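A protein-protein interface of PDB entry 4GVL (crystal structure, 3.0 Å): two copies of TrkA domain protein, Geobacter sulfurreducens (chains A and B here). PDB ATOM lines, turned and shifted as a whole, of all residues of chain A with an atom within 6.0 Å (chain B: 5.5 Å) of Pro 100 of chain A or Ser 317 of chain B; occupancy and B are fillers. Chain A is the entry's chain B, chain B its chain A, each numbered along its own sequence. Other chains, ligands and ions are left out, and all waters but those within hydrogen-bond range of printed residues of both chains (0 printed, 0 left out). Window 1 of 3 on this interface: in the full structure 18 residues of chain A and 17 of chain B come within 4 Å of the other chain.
The side-chain carboxylate of Asp 101 of chain A lies within hydrogen-bond range of the side-chain hydroxyl of Ser 317 of chain B (2.7 Å).
The side-chain hydroxyl (OG) of Ser 317 of chain B lies within hydrogen-bond range of the side-chain amide nitrogen (ND2) of Asn 104 of chain A (3.1 Å).
N of Asp 101 of chain A is in hydrogen-bond range of OG of Ser 98 of chain A, 3.0 Å away.
Among the printed residues, pairs that only touch across the chains: Asp 99 of chain A with Phe 321 of chain B, Pro 100 of chain A with Ser 317 of chain B, Pro 100 of chain A with Phe 321 of chain B and Asn 104 of chain A with Ile 320 of chain B.
Thr 77 of chain A touches none of the printed residues of chain B.
Of the printed residues of chain B, Asp 99 of chain A touches Phe 321 (3.9 Å).
Of the printed residues of chain B, Asp 101 of chain A touches Ser 317.
Of the printed residues of chain B, Asn 104 of chain A touches Ser 317 and Ile 320.
Ser 317 of chain B touches just these residues of chain A: Pro 100 (3.6 Å), Asp 101 (2.7 Å) and Asn 104 (3.1 Å).
Of the printed residues of chain A, Ile 320 of chain B touches Asn 104.
Printed residues of chain A within 4 Å of Phe 321 of chain B: Asp 99 (3.9 Å) and Pro 100 (3.6 Å).
The nearest residue of chain A that does not touch Ser 317 of chain B is Thr 77 of chain A (4.6 Å).
The nearest printed residue of chain B that does not touch Asp 101 of chain A is Asp 315 of chain B (5.0 Å).
Hydrophobic or aromatic side chains of chain B that line the printed part of chain A: Ile 320 and Phe 321.
Hydrophobic or aromatic side chains of chain A within 4 Å of the printed part of chain B: Pro 100.
Among the printed residues, 6 pairs touch across the chains.
No position is printed for both chains.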
ATOM      1  N   THR A  77       8.504  -3.938 -18.763  1.00  0.00           N
ATOM      2  CA  THR A  77       8.637  -2.579 -19.265  1.00  0.00           C
ATOM      3  C   THR A  77       9.510  -2.489 -20.501  1.00  0.00           C
ATOM      4  O   THR A  77       9.765  -1.396 -21.014  1.00  0.00           O
ATOM      5  CB  THR A  77       9.113  -1.622 -18.161  1.00  0.00           C
ATOM      6  OG1 THR A  77      10.113  -2.276 -17.366  1.00  0.00           O
ATOM      7  CG2 THR A  77       7.937  -1.231 -17.266  1.00  0.00           C
ATOM      8  N   SER A  98       3.648  -1.054  -9.244  1.00  0.00           N
ATOM      9  CA  SER A  98       3.887   0.182  -8.524  1.00  0.00           C
ATOM     10  C   SER A  98       3.464   1.332  -9.424  1.00  0.00           C
ATOM     11  O   SER A  98       3.294   1.151 -10.634  1.00  0.00           O
ATOM     12  CB  SER A  98       5.357   0.300  -8.152  1.00  0.00           C
ATOM     13  OG  SER A  98       6.131   0.772  -9.237  1.00  0.00           O
ATOM     14  N   ASP A  99       3.271   2.514  -8.862  1.00  0.00           N
ATOM     15  CA  ASP A  99       2.833   3.601  -9.713  1.00  0.00           C
ATOM     16  C   ASP A  99       3.859   4.004 -10.759  1.00  0.00           C
ATOM     17  O   ASP A  99       3.501   4.186 -11.922  1.00  0.00           O
ATOM     18  CB  ASP A  99       2.296   4.771  -8.911  1.00  0.00           C
ATOM     19  CG  ASP A  99       0.895   4.505  -8.423  1.00  0.00           C
ATOM     20  OD1 ASP A  99       0.293   5.406  -7.773  1.00  0.00           O
ATOM     21  OD2 ASP A  99       0.396   3.377  -8.708  1.00  0.00           O
ATOM     22  N   PRO A 100       5.141   4.117 -10.370  1.00  0.00           N
ATOM     23  CA  PRO A 100       6.110   4.395 -11.408  1.00  0.00           C
ATOM     24  C   PRO A 100       6.114   3.286 -12.444  1.00  0.00           C
ATOM     25  O   PRO A 100       5.993   3.570 -13.625  1.00  0.00           O
ATOM     26  CB  PRO A 100       7.426   4.445 -10.636  1.00  0.00           C
ATOM     27  CG  PRO A 100       7.009   4.859  -9.270  1.00  0.00           C
ATOM     28  CD  PRO A 100       5.794   4.039  -9.054  1.00  0.00           C
ATOM     29  N   ASP A 101       6.202   2.032 -12.010  1.00  0.00           N
ATOM     30  CA  ASP A 101       6.201   0.913 -12.954  1.00  0.00           C
ATOM     31  C   ASP A 101       4.984   0.927 -13.876  1.00  0.00           C
ATOM     32  O   ASP A 101       5.087   0.546 -15.040  1.00  0.00           O
ATOM     33  CB  ASP A 101       6.331  -0.436 -12.244  1.00  0.00           C
ATOM     34  CG  ASP A 101       7.775  -0.778 -11.900  1.00  0.00           C
ATOM     35  OD1 ASP A 101       8.655   0.091 -12.074  1.00  0.00           O
ATOM     36  OD2 ASP A 101       8.043  -1.922 -11.464  1.00  0.00           O
ATOM     37  N   ASN A 102       3.840   1.385 -13.377  1.00  0.00           N
ATOM     38  CA  ASN A 102       2.661   1.460 -14.229  1.00  0.00           C
ATOM     39  C   ASN A 102       2.812   2.497 -15.336  1.00  0.00           C
ATOM     40  O   ASN A 102       2.538   2.211 -16.483  1.00  0.00           O
ATOM     41  CB  ASN A 102       1.382   1.658 -13.405  1.00  0.00           C
ATOM     42  CG  ASN A 102       0.806   0.345 -12.913  1.00  0.00           C
ATOM     43  OD1 ASN A 102       1.457  -0.697 -12.973  1.00  0.00           O
ATOM     44  ND2 ASN A 102      -0.418   0.387 -12.433  1.00  0.00           N
ATOM     45  N   ALA A 103       3.284   3.685 -14.989  1.00  0.00           N
ATOM     46  CA  ALA A 103       3.525   4.732 -15.970  1.00  0.00           C
ATOM     47  C   ALA A 103       4.427   4.204 -17.066  1.00  0.00           C
ATOM     48  O   ALA A 103       4.150   4.399 -18.247  1.00  0.00           O
ATOM     49  CB  ALA A 103       4.156   5.936 -15.311  1.00  0.00           C
ATOM     50  N   ASN A 104       5.497   3.525 -16.661  1.00  0.00           N
ATOM     51  CA  ASN A 104       6.471   2.961 -17.585  1.00  0.00           C
ATOM     52  C   ASN A 104       5.785   1.947 -18.489  1.00  0.00           C
ATOM     53  O   ASN A 104       5.941   1.987 -19.704  1.00  0.00           O
ATOM     54  CB  ASN A 104       7.633   2.323 -16.801  1.00  0.00           C
ATOM     55  CG  ASN A 104       8.844   1.973 -17.675  1.00  0.00           C
ATOM     56  OD1 ASN A 104       8.973   2.436 -18.799  1.00  0.00           O
ATOM     57  ND2 ASN A 104       9.736   1.160 -17.140  1.00  0.00           N
ATOM     58  N   LEU A 105       4.998   1.066 -17.884  1.00  0.00           N
ATOM     59  CA  LEU A 105       4.226   0.069 -18.625  1.00  0.00           C
ATOM     60  C   LEU A 105       3.345   0.732 -19.690  1.00  0.00           C
ATOM     61  O   LEU A 105       3.507   0.469 -20.881  1.00  0.00           O
ATOM     62  CB  LEU A 105       3.380  -0.771 -17.673  1.00  0.00           C
ATOM     63  CG  LEU A 105       2.546  -1.830 -18.367  1.00  0.00           C
ATOM     64  CD1 LEU A 105       3.432  -2.698 -19.212  1.00  0.00           C
ATOM     65  CD2 LEU A 105       1.838  -2.666 -17.348  1.00  0.00           C
ATOM     66  N   THR B 293       9.355  10.862  -5.450  1.00  0.00           N
ATOM     67  CA  THR B 293       8.086  10.176  -5.697  1.00  0.00           C
ATOM     68  C   THR B 293       6.944  10.617  -4.792  1.00  0.00           C
ATOM     69  O   THR B 293       5.818  10.780  -5.250  1.00  0.00           O
ATOM     70  CB  THR B 293       8.308   8.665  -5.529  1.00  0.00           C
ATOM     71  OG1 THR B 293       9.169   8.206  -6.577  1.00  0.00           O
ATOM     72  CG2 THR B 293       6.994   7.866  -5.528  1.00  0.00           C
ATOM     73  N   ASP B 315      16.914   4.131 -11.064  1.00  0.00           N
ATOM     74  CA  ASP B 315      15.797   3.243 -11.433  1.00  0.00           C
ATOM     75  C   ASP B 315      14.910   3.926 -12.465  1.00  0.00           C
ATOM     76  O   ASP B 315      14.378   5.005 -12.217  1.00  0.00           O
ATOM     77  CB  ASP B 315      14.995   2.845 -10.195  1.00  0.00           C
ATOM     78  CG  ASP B 315      13.731   2.088 -10.532  1.00  0.00           C
ATOM     79  OD1 ASP B 315      12.702   2.759 -10.736  1.00  0.00           O
ATOM     80  OD2 ASP B 315      13.750   0.830 -10.560  1.00  0.00           O
ATOM     81  N   ASP B 316      14.746   3.299 -13.627  1.00  0.00           N
ATOM     82  CA  ASP B 316      14.148   3.997 -14.770  1.00  0.00           C
ATOM     83  C   ASP B 316      12.683   4.375 -14.624  1.00  0.00           C
ATOM     84  O   ASP B 316      12.312   5.519 -14.941  1.00  0.00           O
ATOM     85  CB  ASP B 316      14.362   3.219 -16.062  1.00  0.00           C
ATOM     86  CG  ASP B 316      15.640   3.610 -16.770  1.00  0.00           C
ATOM     87  OD1 ASP B 316      16.130   4.769 -16.582  1.00  0.00           O
ATOM     88  OD2 ASP B 316      16.146   2.749 -17.520  1.00  0.00           O
ATOM     89  N   SER B 317      11.856   3.434 -14.155  1.00  0.00           N
ATOM     90  CA  SER B 317      10.456   3.733 -13.911  1.00  0.00           C
ATOM     91  C   SER B 317      10.290   4.947 -13.014  1.00  0.00           C
ATOM     92  O   SER B 317       9.422   5.780 -13.264  1.00  0.00           O
ATOM     93  CB  SER B 317       9.740   2.552 -13.314  1.00  0.00           C
ATOM     94  OG  SER B 317      10.021   1.392 -14.055  1.00  0.00           O
ATOM     95  N   THR B 318      11.138   5.074 -11.995  1.00  0.00           N
ATOM     96  CA  THR B 318      11.120   6.250 -11.139  1.00  0.00           C
ATOM     97  C   THR B 318      11.314   7.523 -11.941  1.00  0.00           C
ATOM     98  O   THR B 318      10.537   8.479 -11.797  1.00  0.00           O
ATOM     99  CB  THR B 318      12.209   6.198 -10.099  1.00  0.00           C
ATOM    100  OG1 THR B 318      12.082   4.995  -9.340  1.00  0.00           O
ATOM    101  CG2 THR B 318      12.129   7.417  -9.187  1.00  0.00           C
ATOM    102  N   ASN B 319      12.352   7.535 -12.782  1.00  0.00           N
ATOM    103  CA  ASN B 319      12.667   8.714 -13.581  1.00  0.00           C
ATOM    104  C   ASN B 319      11.587   9.005 -14.611  1.00  0.00           C
ATOM    105  O   ASN B 319      11.346  10.174 -14.953  1.00  0.00           O
ATOM    106  CB  ASN B 319      13.997   8.564 -14.301  1.00  0.00           C
ATOM    107  CG  ASN B 319      15.138   8.238 -13.370  1.00  0.00           C
ATOM    108  OD1 ASN B 319      15.324   7.086 -12.992  1.00  0.00           O
ATOM    109  ND2 ASN B 319      15.936   9.237 -13.034  1.00  0.00           N
ATOM    110  N   ILE B 320      10.939   7.950 -15.114  1.00  0.00           N
ATOM    111  CA  ILE B 320       9.800   8.153 -15.999  1.00  0.00           C
ATOM    112  C   ILE B 320       8.673   8.824 -15.217  1.00  0.00           C
ATOM    113  O   ILE B 320       8.125   9.861 -15.634  1.00  0.00           O
ATOM    114  CB  ILE B 320       9.327   6.862 -16.647  1.00  0.00           C
ATOM    115  CG1 ILE B 320      10.358   6.400 -17.672  1.00  0.00           C
ATOM    116  CG2 ILE B 320       8.025   7.099 -17.366  1.00  0.00           C
ATOM    117  CD1 ILE B 320      10.167   4.984 -18.138  1.00  0.00           C
ATOM    118  N   PHE B 321       8.369   8.255 -14.058  1.00  0.00           N
ATOM    119  CA  PHE B 321       7.342   8.802 -13.190  1.00  0.00           C
ATOM    120  C   PHE B 321       7.598  10.275 -12.841  1.00  0.00           C
ATOM    121  O   PHE B 321       6.664  11.079 -12.754  1.00  0.00           O
ATOM    122  CB  PHE B 321       7.266   7.962 -11.929  1.00  0.00           C
ATOM    123  CG  PHE B 321       6.154   8.334 -11.035  1.00  0.00           C
ATOM    124  CD1 PHE B 321       4.893   7.788 -11.225  1.00  0.00           C
ATOM    125  CD2 PHE B 321       6.359   9.235  -9.994  1.00  0.00           C
ATOM    126  CE1 PHE B 321       3.833   8.138 -10.387  1.00  0.00           C
ATOM    127  CE2 PHE B 321       5.322   9.599  -9.147  1.00  0.00           C
ATOM    128  CZ  PHE B 321       4.051   9.050  -9.341  1.00  0.00           C
ATOM    129  N   LEU B 322       8.870  10.626 -12.652  1.00  0.00           N
ATOM    130  CA  LEU B 322       9.215  11.944 -12.133  1.00  0.00           C
ATOM    131  C   LEU B 322       9.136  12.998 -13.222  1.00  0.00           C
ATOM    132  O   LEU B 322       8.737  14.151 -12.972  1.00  0.00           O
ATOM    133  CB  LEU B 322      10.600  11.912 -11.503  1.00  0.00           C
ATOM    134  CG  LEU B 322      10.640  11.309 -10.105  1.00  0.00           C
ATOM    135  CD1 LEU B 322      12.069  11.302  -9.603  1.00  0.00           C
ATOM    136  CD2 LEU B 322       9.709  12.050  -9.131  1.00  0.00           C
